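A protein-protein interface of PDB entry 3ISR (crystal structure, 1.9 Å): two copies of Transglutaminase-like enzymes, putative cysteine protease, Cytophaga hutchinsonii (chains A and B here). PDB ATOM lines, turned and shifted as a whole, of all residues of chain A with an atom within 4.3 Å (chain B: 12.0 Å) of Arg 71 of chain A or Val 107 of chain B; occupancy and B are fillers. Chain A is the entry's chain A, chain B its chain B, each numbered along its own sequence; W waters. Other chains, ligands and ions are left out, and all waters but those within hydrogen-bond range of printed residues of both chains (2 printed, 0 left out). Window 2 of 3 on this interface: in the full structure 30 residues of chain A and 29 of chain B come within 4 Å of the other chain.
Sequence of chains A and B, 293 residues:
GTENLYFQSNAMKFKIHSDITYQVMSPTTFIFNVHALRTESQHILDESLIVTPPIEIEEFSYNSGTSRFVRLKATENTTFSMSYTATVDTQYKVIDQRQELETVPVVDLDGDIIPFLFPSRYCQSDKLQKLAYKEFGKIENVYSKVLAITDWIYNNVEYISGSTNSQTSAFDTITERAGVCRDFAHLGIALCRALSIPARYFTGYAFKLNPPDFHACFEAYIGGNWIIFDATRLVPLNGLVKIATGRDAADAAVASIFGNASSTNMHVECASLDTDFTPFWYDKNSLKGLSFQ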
ATOM      1  N   THR A  29      32.208 -16.910 -15.807  1.00  0.00           N
ATOM      2  CA  THR A  29      31.018 -17.685 -15.467  1.00  0.00           C
ATOM      3  C   THR A  29      31.423 -19.084 -14.999  1.00  0.00           C
ATOM      4  O   THR A  29      32.298 -19.718 -15.588  1.00  0.00           O
ATOM      5  CB  THR A  29      30.026 -17.756 -16.667  1.00  0.00           C
ATOM      6  OG1 THR A  29      29.428 -16.466 -16.845  1.00  0.00           O
ATOM      7  CG2 THR A  29      28.906 -18.759 -16.391  1.00  0.00           C
ATOM      8  N   PHE A  30      30.793 -19.545 -13.924  1.00  0.00           N
ATOM      9  CA  PHE A  30      31.048 -20.871 -13.375  1.00  0.00           C
ATOM     10  C   PHE A  30      29.817 -21.733 -13.470  1.00  0.00           C
ATOM     11  O   PHE A  30      28.712 -21.264 -13.191  1.00  0.00           O
ATOM     12  CB  PHE A  30      31.375 -20.754 -11.879  1.00  0.00           C
ATOM     13  CG  PHE A  30      32.631 -20.029 -11.595  1.00  0.00           C
ATOM     14  CD1 PHE A  30      33.802 -20.730 -11.354  1.00  0.00           C
ATOM     15  CD2 PHE A  30      32.659 -18.646 -11.574  1.00  0.00           C
ATOM     16  CE1 PHE A  30      34.999 -20.047 -11.082  1.00  0.00           C
ATOM     17  CE2 PHE A  30      33.844 -17.958 -11.304  1.00  0.00           C
ATOM     18  CZ  PHE A  30      35.011 -18.667 -11.060  1.00  0.00           C
ATOM     19  N   ILE A  31      30.005 -22.998 -13.842  1.00  0.00           N
ATOM     20  CA  ILE A  31      28.957 -24.000 -13.680  1.00  0.00           C
ATOM     21  C   ILE A  31      29.480 -25.087 -12.744  1.00  0.00           C
ATOM     22  O   ILE A  31      30.491 -25.753 -13.043  1.00  0.00           O
ATOM     23  CB  ILE A  31      28.502 -24.629 -15.019  1.00  0.00           C
ATOM     24  CG1 ILE A  31      28.117 -23.521 -16.015  1.00  0.00           C
ATOM     25  CG2 ILE A  31      27.275 -25.555 -14.776  1.00  0.00           C
ATOM     26  CD1 ILE A  31      27.731 -24.039 -17.397  1.00  0.00           C
ATOM     27  N   GLU A  56      24.512 -13.831  -7.193  1.00  0.00           N
ATOM     28  CA  GLU A  56      23.303 -14.455  -7.707  1.00  0.00           C
ATOM     29  C   GLU A  56      23.660 -15.833  -8.274  1.00  0.00           C
ATOM     30  O   GLU A  56      24.617 -15.964  -9.039  1.00  0.00           O
ATOM     31  CB  GLU A  56      22.654 -13.590  -8.781  1.00  0.00           C
ATOM     32  CG  GLU A  56      21.360 -14.189  -9.340  1.00  0.00           C
ATOM     33  CD  GLU A  56      20.714 -13.316 -10.403  1.00  0.00           C
ATOM     34  OE1 GLU A  56      20.050 -12.330 -10.038  1.00  0.00           O
ATOM     35  OE2 GLU A  56      20.872 -13.614 -11.604  1.00  0.00           O
ATOM     36  N   ILE A  57      22.888 -16.842  -7.891  1.00  0.00           N
ATOM     37  CA  ILE A  57      23.160 -18.232  -8.285  1.00  0.00           C
ATOM     38  C   ILE A  57      21.855 -18.918  -8.738  1.00  0.00           C
ATOM     39  O   ILE A  57      20.789 -18.664  -8.184  1.00  0.00           O
ATOM     40  CB  ILE A  57      23.922 -18.993  -7.139  1.00  0.00           C
ATOM     41  CG1 ILE A  57      24.557 -20.294  -7.651  1.00  0.00           C
ATOM     42  CG2 ILE A  57      23.012 -19.228  -5.888  1.00  0.00           C
ATOM     43  CD1 ILE A  57      25.629 -20.891  -6.696  1.00  0.00           C
ATOM     44  N   GLU A  58      21.934 -19.742  -9.779  1.00  0.00           N
ATOM     45  CA  GLU A  58      20.745 -20.362 -10.350  1.00  0.00           C
ATOM     46  C   GLU A  58      20.979 -21.855 -10.548  1.00  0.00           C
ATOM     47  O   GLU A  58      21.989 -22.253 -11.136  1.00  0.00           O
ATOM     48  CB  GLU A  58      20.393 -19.712 -11.698  1.00  0.00           C
ATOM     49  CG  GLU A  58      19.154 -20.311 -12.356  1.00  0.00           C
ATOM     50  CD  GLU A  58      19.287 -20.442 -13.867  1.00  0.00           C
ATOM     51  OE1 GLU A  58      19.543 -21.569 -14.350  1.00  0.00           O
ATOM     52  OE2 GLU A  58      19.143 -19.430 -14.574  1.00  0.00           O
ATOM     53  N   PHE A  60      20.062 -25.419 -12.373  1.00  0.00           N
ATOM     54  CA  PHE A  60      19.420 -25.993 -13.569  1.00  0.00           C
ATOM     55  C   PHE A  60      19.883 -27.440 -13.805  1.00  0.00           C
ATOM     56  O   PHE A  60      20.910 -27.878 -13.275  1.00  0.00           O
ATOM     57  CB  PHE A  60      19.723 -25.138 -14.817  1.00  0.00           C
ATOM     58  CG  PHE A  60      21.119 -25.310 -15.343  1.00  0.00           C
ATOM     59  CD1 PHE A  60      22.185 -24.597 -14.780  1.00  0.00           C
ATOM     60  CD2 PHE A  60      21.378 -26.194 -16.398  1.00  0.00           C
ATOM     61  CE1 PHE A  60      23.478 -24.758 -15.250  1.00  0.00           C
ATOM     62  CE2 PHE A  60      22.673 -26.366 -16.884  1.00  0.00           C
ATOM     63  CZ  PHE A  60      23.732 -25.653 -16.313  1.00  0.00           C
ATOM     64  N   VAL A  70      24.716 -25.701 -10.564  1.00  0.00           N
ATOM     65  CA  VAL A  70      24.476 -24.299 -10.203  1.00  0.00           C
ATOM     66  C   VAL A  70      25.413 -23.395 -10.977  1.00  0.00           C
ATOM     67  O   VAL A  70      26.577 -23.724 -11.185  1.00  0.00           O
ATOM     68  CB  VAL A  70      24.593 -24.009  -8.696  1.00  0.00           C
ATOM     69  CG1 VAL A  70      23.418 -24.615  -7.967  1.00  0.00           C
ATOM     70  CG2 VAL A  70      25.895 -24.534  -8.145  1.00  0.00           C
ATOM     71  N   ARG A  71      24.905 -22.260 -11.416  1.00  0.00           N
ATOM     72  CA  ARG A  71      25.736 -21.344 -12.171  1.00  0.00           C
ATOM     73  C   ARG A  71      25.674 -19.921 -11.635  1.00  0.00           C
ATOM     74  O   ARG A  71      24.643 -19.470 -11.101  1.00  0.00           O
ATOM     75  CB  ARG A  71      25.437 -21.396 -13.664  1.00  0.00           C
ATOM     76  CG  ARG A  71      23.996 -21.226 -14.015  1.00  0.00           C
ATOM     77  CD  ARG A  71      23.838 -21.112 -15.522  1.00  0.00           C
ATOM     78  NE  ARG A  71      22.428 -21.202 -15.866  1.00  0.00           N
ATOM     79  CZ  ARG A  71      21.956 -21.342 -17.094  1.00  0.00           C
ATOM     80  NH1 ARG A  71      20.650 -21.401 -17.278  1.00  0.00           N
ATOM     81  NH2 ARG A  71      22.782 -21.400 -18.133  1.00  0.00           N
ATOM     82  N   LEU A  72      26.809 -19.240 -11.763  1.00  0.00           N
ATOM     83  CA  LEU A  72      26.933 -17.863 -11.308  1.00  0.00           C
ATOM     84  C   LEU A  72      28.001 -17.182 -12.149  1.00  0.00           C
ATOM     85  O   LEU A  72      28.804 -17.858 -12.798  1.00  0.00           O
ATOM     86  CB  LEU A  72      27.268 -17.820  -9.797  1.00  0.00           C
ATOM     87  CG  LEU A  72      28.592 -18.374  -9.235  1.00  0.00           C
ATOM     88  CD1 LEU A  72      29.768 -17.467  -9.534  1.00  0.00           C
ATOM     89  CD2 LEU A  72      28.498 -18.547  -7.738  1.00  0.00           C
ATOM     90  N   LYS A  73      27.995 -15.852 -12.165  1.00  0.00           N
ATOM     91  CA  LYS A  73      29.069 -15.104 -12.811  1.00  0.00           C
ATOM     92  C   LYS A  73      29.756 -14.201 -11.803  1.00  0.00           C
ATOM     93  O   LYS A  73      29.098 -13.607 -10.943  1.00  0.00           O
ATOM     94  CB  LYS A  73      28.563 -14.293 -14.011  1.00  0.00           C
ATOM     95  CG  LYS A  73      27.431 -13.330 -13.693  1.00  0.00           C
ATOM     96  CD  LYS A  73      26.958 -12.597 -14.937  1.00  0.00           C
ATOM     97  CE  LYS A  73      25.742 -11.725 -14.616  1.00  0.00           C
ATOM     98  NZ  LYS A  73      25.281 -10.931 -15.799  1.00  0.00           N
ATOM     99  N   LEU B 101      26.738 -10.357 -30.754  1.00  0.00           N
ATOM    100  CA  LEU B 101      27.391 -10.175 -29.454  1.00  0.00           C
ATOM    101  C   LEU B 101      28.898 -10.415 -29.580  1.00  0.00           C
ATOM    102  O   LEU B 101      29.353 -11.043 -30.544  1.00  0.00           O
ATOM    103  CB  LEU B 101      26.772 -11.139 -28.429  1.00  0.00           C
ATOM    104  N   THR B 103      30.491 -12.152 -27.256  1.00  0.00           N
ATOM    105  CA  THR B 103      30.545 -13.553 -26.802  1.00  0.00           C
ATOM    106  C   THR B 103      29.141 -14.152 -26.561  1.00  0.00           C
ATOM    107  O   THR B 103      28.144 -13.426 -26.532  1.00  0.00           O
ATOM    108  CB  THR B 103      31.378 -13.712 -25.502  1.00  0.00           C
ATOM    109  OG1 THR B 103      30.871 -12.835 -24.485  1.00  0.00           O
ATOM    110  CG2 THR B 103      32.868 -13.410 -25.743  1.00  0.00           C
ATOM    111  N   VAL B 104      29.072 -15.475 -26.381  1.00  0.00           N
ATOM    112  CA  VAL B 104      27.811 -16.145 -25.995  1.00  0.00           C
ATOM    113  C   VAL B 104      27.618 -16.060 -24.460  1.00  0.00           C
ATOM    114  O   VAL B 104      28.528 -16.449 -23.701  1.00  0.00           O
ATOM    115  CB  VAL B 104      27.744 -17.632 -26.513  1.00  0.00           C
ATOM    116  CG1 VAL B 104      26.560 -18.405 -25.889  1.00  0.00           C
ATOM    117  CG2 VAL B 104      27.629 -17.667 -28.041  1.00  0.00           C
ATOM    118  N   PRO B 105      26.450 -15.551 -23.996  1.00  0.00           N
ATOM    119  CA  PRO B 105      26.233 -15.333 -22.546  1.00  0.00           C
ATOM    120  C   PRO B 105      25.910 -16.642 -21.792  1.00  0.00           C
ATOM    121  O   PRO B 105      24.737 -16.949 -21.543  1.00  0.00           O
ATOM    122  CB  PRO B 105      25.023 -14.398 -22.532  1.00  0.00           C
ATOM    123  CG  PRO B 105      24.224 -14.856 -23.732  1.00  0.00           C
ATOM    124  CD  PRO B 105      25.247 -15.196 -24.783  1.00  0.00           C
ATOM    125  N   VAL B 106      26.953 -17.396 -21.440  1.00  0.00           N
ATOM    126  CA  VAL B 106      26.795 -18.742 -20.876  1.00  0.00           C
ATOM    127  C   VAL B 106      25.860 -18.773 -19.669  1.00  0.00           C
ATOM    128  O   VAL B 106      25.014 -19.657 -19.559  1.00  0.00           O
ATOM    129  CB  VAL B 106      28.157 -19.410 -20.546  1.00  0.00           C
ATOM    130  CG1 VAL B 106      27.950 -20.768 -19.892  1.00  0.00           C
ATOM    131  CG2 VAL B 106      28.972 -19.593 -21.804  1.00  0.00           C
ATOM    132  N   VAL B 107      25.991 -17.785 -18.784  1.00  0.00           N
ATOM    133  CA  VAL B 107      25.188 -17.751 -17.581  1.00  0.00           C
ATOM    134  C   VAL B 107      23.678 -17.723 -17.881  1.00  0.00           C
ATOM    135  O   VAL B 107      22.880 -18.121 -17.033  1.00  0.00           O
ATOM    136  CB  VAL B 107      25.628 -16.607 -16.624  1.00  0.00           C
ATOM    137  CG1 VAL B 107      25.097 -15.220 -17.069  1.00  0.00           C
ATOM    138  CG2 VAL B 107      25.228 -16.921 -15.175  1.00  0.00           C
ATOM    139  N   ASP B 108      23.306 -17.290 -19.091  1.00  0.00           N
ATOM    140  CA  ASP B 108      21.894 -17.074 -19.455  1.00  0.00           C
ATOM    141  C   ASP B 108      21.303 -18.099 -20.432  1.00  0.00           C
ATOM    142  O   ASP B 108      20.099 -18.054 -20.712  1.00  0.00           O
ATOM    143  CB  ASP B 108      21.706 -15.666 -20.033  1.00  0.00           C
ATOM    144  CG  ASP B 108      21.942 -14.564 -18.994  1.00  0.00           C
ATOM    145  OD1 ASP B 108      21.538 -14.735 -17.821  1.00  0.00           O
ATOM    146  OD2 ASP B 108      22.540 -13.525 -19.355  1.00  0.00           O
ATOM    147  N   LEU B 109      22.136 -19.007 -20.951  1.00  0.00           N
ATOM    148  CA  LEU B 109      21.666 -20.035 -21.888  1.00  0.00           C
ATOM    149  C   LEU B 109      20.652 -20.976 -21.244  1.00  0.00           C
ATOM    150  O   LEU B 109      20.801 -21.348 -20.067  1.00  0.00           O
ATOM    151  CB  LEU B 109      22.841 -20.858 -22.427  1.00  0.00           C
ATOM    152  CG  LEU B 109      23.861 -20.122 -23.303  1.00  0.00           C
ATOM    153  CD1 LEU B 109      25.046 -21.001 -23.631  1.00  0.00           C
ATOM    154  CD2 LEU B 109      23.191 -19.586 -24.600  1.00  0.00           C
ATOM    155  N   ASP B 110      19.633 -21.366 -22.012  1.00  0.00           N
ATOM    156  CA  ASP B 110      18.721 -22.432 -21.589  1.00  0.00           C
ATOM    157  C   ASP B 110      19.550 -23.671 -21.257  1.00  0.00           C
ATOM    158  O   ASP B 110      20.540 -23.962 -21.925  1.00  0.00           O
ATOM    159  CB  ASP B 110      17.729 -22.791 -22.699  1.00  0.00           C
ATOM    160  CG  ASP B 110      16.623 -21.741 -22.892  1.00  0.00           C
ATOM    161  OD1 ASP B 110      16.584 -20.699 -22.201  1.00  0.00           O
ATOM    162  OD2 ASP B 110      15.766 -21.972 -23.762  1.00  0.00           O
ATOM    163  N   GLY B 111      19.139 -24.392 -20.219  1.00  0.00           N
ATOM    164  CA  GLY B 111      19.839 -25.578 -19.760  1.00  0.00           C
ATOM    165  C   GLY B 111      20.044 -26.612 -20.850  1.00  0.00           C
ATOM    166  O   GLY B 111      21.076 -27.299 -20.869  1.00  0.00           O
ATOM    167  N   ASP B 112      19.084 -26.728 -21.772  1.00  0.00           N
ATOM    168  CA  ASP B 112      19.254 -27.674 -22.879  1.00  0.00           C
ATOM    169  C   ASP B 112      20.290 -27.291 -23.954  1.00  0.00           C
ATOM    170  O   ASP B 112      20.641 -28.118 -24.818  1.00  0.00           O
ATOM    171  CB  ASP B 112      17.901 -28.126 -23.474  1.00  0.00           C
ATOM    172  CG  ASP B 112      17.184 -27.054 -24.304  1.00  0.00           C
ATOM    173  OD1 ASP B 112      17.560 -25.859 -24.301  1.00  0.00           O
ATOM    174  OD2 ASP B 112      16.191 -27.433 -24.970  1.00  0.00           O
ATOM    175  N   ILE B 113      20.800 -26.066 -23.883  1.00  0.00           N
ATOM    176  CA  ILE B 113      21.884 -25.622 -24.794  1.00  0.00           C
ATOM    177  C   ILE B 113      23.262 -25.948 -24.218  1.00  0.00           C
ATOM    178  O   ILE B 113      24.190 -26.264 -24.947  1.00  0.00           O
ATOM    179  CB  ILE B 113      21.796 -24.102 -25.068  1.00  0.00           C
ATOM    180  CG1 ILE B 113      20.380 -23.716 -25.509  1.00  0.00           C
ATOM    181  CG2 ILE B 113      22.831 -23.639 -26.106  1.00  0.00           C
ATOM    182  CD1 ILE B 113      19.878 -24.467 -26.708  1.00  0.00           C
ATOM    183  N   ILE B 114      23.367 -25.904 -22.896  1.00  0.00           N
ATOM    184  CA  ILE B 114      24.655 -26.046 -22.205  1.00  0.00           C
ATOM    185  C   ILE B 114      25.486 -27.259 -22.646  1.00  0.00           C
ATOM    186  O   ILE B 114      26.685 -27.114 -22.833  1.00  0.00           O
ATOM    187  CB  ILE B 114      24.463 -26.030 -20.673  1.00  0.00           C
ATOM    188  CG1 ILE B 114      23.873 -24.680 -20.233  1.00  0.00           C
ATOM    189  CG2 ILE B 114      25.787 -26.347 -19.943  1.00  0.00           C
ATOM    190  CD1 ILE B 114      24.792 -23.494 -20.439  1.00  0.00           C
ATOM    191  N   PRO B 115      24.862 -28.446 -22.806  1.00  0.00           N
ATOM    192  CA  PRO B 115      25.661 -29.625 -23.181  1.00  0.00           C
ATOM    193  C   PRO B 115      26.483 -29.433 -24.456  1.00  0.00           C
ATOM    194  O   PRO B 115      27.538 -30.052 -24.605  1.00  0.00           O
ATOM    195  CB  PRO B 115      24.593 -30.719 -23.381  1.00  0.00           C
ATOM    196  CG  PRO B 115      23.488 -30.306 -22.487  1.00  0.00           C
ATOM    197  CD  PRO B 115      23.451 -28.810 -22.556  1.00  0.00           C
ATOM    198  N   PHE B 116      26.043 -28.534 -25.341  1.00  0.00           N
ATOM    199  CA  PHE B 116      26.701 -28.354 -26.623  1.00  0.00           C
ATOM    200  C   PHE B 116      27.916 -27.434 -26.549  1.00  0.00           C
ATOM    201  O   PHE B 116      28.523 -27.103 -27.556  1.00  0.00           O
ATOM    202  CB  PHE B 116      25.671 -27.926 -27.681  1.00  0.00           C
ATOM    203  CG  PHE B 116      24.586 -28.947 -27.860  1.00  0.00           C
ATOM    204  CD1 PHE B 116      24.839 -30.117 -28.566  1.00  0.00           C
ATOM    205  CD2 PHE B 116      23.328 -28.772 -27.257  1.00  0.00           C
ATOM    206  CE1 PHE B 116      23.846 -31.104 -28.725  1.00  0.00           C
ATOM    207  CE2 PHE B 116      22.315 -29.759 -27.398  1.00  0.00           C
ATOM    208  CZ  PHE B 116      22.588 -30.930 -28.141  1.00  0.00           C
ATOM    209  N   LEU B 117      28.284 -27.045 -25.329  1.00  0.00           N
ATOM    210  CA  LEU B 117      29.547 -26.364 -25.088  1.00  0.00           C
ATOM    211  C   LEU B 117      30.684 -27.357 -24.790  1.00  0.00           C
ATOM    212  O   LEU B 117      31.858 -26.974 -24.752  1.00  0.00           O
ATOM    213  CB  LEU B 117      29.391 -25.404 -23.888  1.00  0.00           C
ATOM    214  CG  LEU B 117      28.569 -24.122 -24.123  1.00  0.00           C
ATOM    215  CD1 LEU B 117      28.111 -23.496 -22.789  1.00  0.00           C
ATOM    216  CD2 LEU B 117      29.376 -23.115 -24.951  1.00  0.00           C
ATOM    217  N   PHE B 118      30.340 -28.615 -24.524  1.00  0.00           N
ATOM    218  CA  PHE B 118      31.311 -29.583 -23.997  1.00  0.00           C
ATOM    219  C   PHE B 118      31.889 -30.513 -25.047  1.00  0.00           C
ATOM    220  O   PHE B 118      31.253 -30.754 -26.078  1.00  0.00           O
ATOM    221  CB  PHE B 118      30.706 -30.357 -22.821  1.00  0.00           C
ATOM    222  CG  PHE B 118      30.449 -29.467 -21.641  1.00  0.00           C
ATOM    223  CD1 PHE B 118      31.493 -29.081 -20.818  1.00  0.00           C
ATOM    224  CD2 PHE B 118      29.187 -28.938 -21.426  1.00  0.00           C
ATOM    225  CE1 PHE B 118      31.268 -28.202 -19.722  1.00  0.00           C
ATOM    226  CE2 PHE B 118      28.940 -28.073 -20.358  1.00  0.00           C
ATOM    227  CZ  PHE B 118      29.972 -27.702 -19.507  1.00  0.00           C
ATOM    228  N   SER B 196      34.018 -21.372 -26.841  1.00  0.00           N
ATOM    229  CA  SER B 196      32.831 -21.185 -25.976  1.00  0.00           C
ATOM    230  C   SER B 196      31.570 -20.805 -26.756  1.00  0.00           C
ATOM    231  O   SER B 196      30.753 -20.009 -26.288  1.00  0.00           O
ATOM    232  CB  SER B 196      33.087 -20.163 -24.857  1.00  0.00           C
ATOM    233  OG  SER B 196      34.284 -20.470 -24.162  1.00  0.00           O
ATOM    234  N   ILE B 197      31.403 -21.386 -27.939  1.00  0.00           N
ATOM    235  CA  ILE B 197      30.187 -21.168 -28.727  1.00  0.00           C
ATOM    236  C   ILE B 197      29.484 -22.528 -28.812  1.00  0.00           C
ATOM    237  O   ILE B 197      30.089 -23.493 -29.282  1.00  0.00           O
ATOM    238  CB  ILE B 197      30.545 -20.652 -30.150  1.00  0.00           C
ATOM    239  CG1 ILE B 197      31.303 -19.330 -30.060  1.00  0.00           C
ATOM    240  CG2 ILE B 197      29.280 -20.472 -31.042  1.00  0.00           C
ATOM    241  CD1 ILE B 197      32.050 -18.971 -31.360  1.00  0.00           C
ATOM    242  N   PRO B 198      28.222 -22.629 -28.349  1.00  0.00           N
ATOM    243  CA  PRO B 198      27.601 -23.946 -28.413  1.00  0.00           C
ATOM    244  C   PRO B 198      27.424 -24.396 -29.857  1.00  0.00           C
ATOM    245  O   PRO B 198      27.096 -23.587 -30.720  1.00  0.00           O
ATOM    246  CB  PRO B 198      26.240 -23.758 -27.719  1.00  0.00           C
ATOM    247  CG  PRO B 198      26.355 -22.440 -26.961  1.00  0.00           C
ATOM    248  CD  PRO B 198      27.341 -21.612 -27.748  1.00  0.00           C
ATOM    249  N   TYR B 221      24.931 -21.996 -31.888  1.00  0.00           N
ATOM    250  CA  TYR B 221      23.872 -21.252 -31.221  1.00  0.00           C
ATOM    251  C   TYR B 221      24.326 -19.827 -31.051  1.00  0.00           C
ATOM    252  O   TYR B 221      25.219 -19.544 -30.241  1.00  0.00           O
ATOM    253  CB  TYR B 221      23.548 -21.883 -29.874  1.00  0.00           C
ATOM    254  CG  TYR B 221      22.295 -21.363 -29.223  1.00  0.00           C
ATOM    255  CD1 TYR B 221      21.032 -21.835 -29.619  1.00  0.00           C
ATOM    256  CD2 TYR B 221      22.362 -20.431 -28.192  1.00  0.00           C
ATOM    257  CE1 TYR B 221      19.856 -21.376 -29.005  1.00  0.00           C
ATOM    258  CE2 TYR B 221      21.183 -19.974 -27.560  1.00  0.00           C
ATOM    259  CZ  TYR B 221      19.948 -20.461 -27.974  1.00  0.00           C
ATOM    260  OH  TYR B 221      18.791 -20.018 -27.360  1.00  0.00           O
HETATM  261  O   HOH W   1      21.624 -18.150 -14.551  1.00  0.00           O
HETATM  262  O   HOH W   2      27.988 -15.857 -18.968  1.00  0.00           O
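Phe 30 of chain A touches none of the printed residues of chain B. Ile 57 of chain A touches none of the printed residues of chain B. Phe 60 of chain A touches just these residues of chain B: Gly 111 (3.7 Å) and Ile 114 (3.9 Å). No residue of chain B comes within 4 Å of Val 70 of chain A. Of chain B, only Val 106 (3.2 Å), Val 107 (3.3 Å), Leu 109 (2.8 Å) and Ile 114 (3.7 Å) come within 4 Å of Arg 71 of chain A. Leu 72 of chain A touches none of the printed residues of chain B. Printed residues of chain A within 4 Å of Val 106 of chain B: Arg 71. Of chain A, only Thr 29, Arg 71 and Lys 73 come within 4 Å of Val 107 of chain B. Of the printed residues of chain A, Leu 109 of chain B touches Arg 71 (2.8 Å). The nearest residue of chain B that does not touch Arg 71 of chain A is Asp 108 of chain B (4.3 Å). The nearest residue of chain A that does not touch Val 107 of chain B is Leu 72 of chain A (4.1 Å). The nearest printed residue of chain A that does not touch Gly 111 of chain B is Arg 71 of chain A (4.5 Å).
The guanidinium group of Arg 71 of chain A is in salt-bridge range of the side-chain carboxylate of Glu 58 of chain A (3.1 Å).
The guanidinium group (NH2) of Arg 71 of chain A sits at hydrogen-bond distance from the backbone carbonyl oxygen (O) of Val 106 of chain B, at 3.2 Å. The backbone carbonyl oxygen (O) of Val 107 of chain B sits at hydrogen-bond distance from the guanidinium group (NE) of Arg 71 of chain A. The guanidinium group (NH2) of Arg 71 of chain A is in hydrogen-bond range of the backbone carbonyl oxygen (O) of Leu 109 of chain B (2.8 Å).
No position is printed for both chains.
Hydrophobic or aromatic side chains of chain B within 4 Å of the printed part of chain A: Val 107 and Ile 114. Of the 11 printed residues of chain A, 5 touch a printed residue of chain B.
Water W2 lies within hydrogen-bond range of the side-chain hydroxyl (OG1) of Thr 29 of chain A, the backbone NH (N) of Val 107 of chain B and the backbone NH (N) of Val 106 of chain B. Water W1 lies within hydrogen-bond range of the backbone carbonyl oxygen (O) of Val 107 of chain B (2.8 Å), the side-chain carboxylate (OE2) of Glu 58 of chain A (2.8 Å) and the guanidinium group (NE) of Arg 71 of chain A (3.4 Å).
Among the printed residues, merely in contact across the chains: Arg 71 of chain A with Ile 114 of chain B (3.7 Å), Phe 60 of chain A with Gly 111 of chain B (3.7 Å), Thr 29 of chain A with Val 107 of chain B (3.8 Å), Lys 73 of chain A with Val 107 of chain B (3.9 Å), Phe 60 of chain A with Ile 114 of chain B (3.9 Å) and Ile 31 of chain A with Ile 114 of chain B (3.9 Å).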
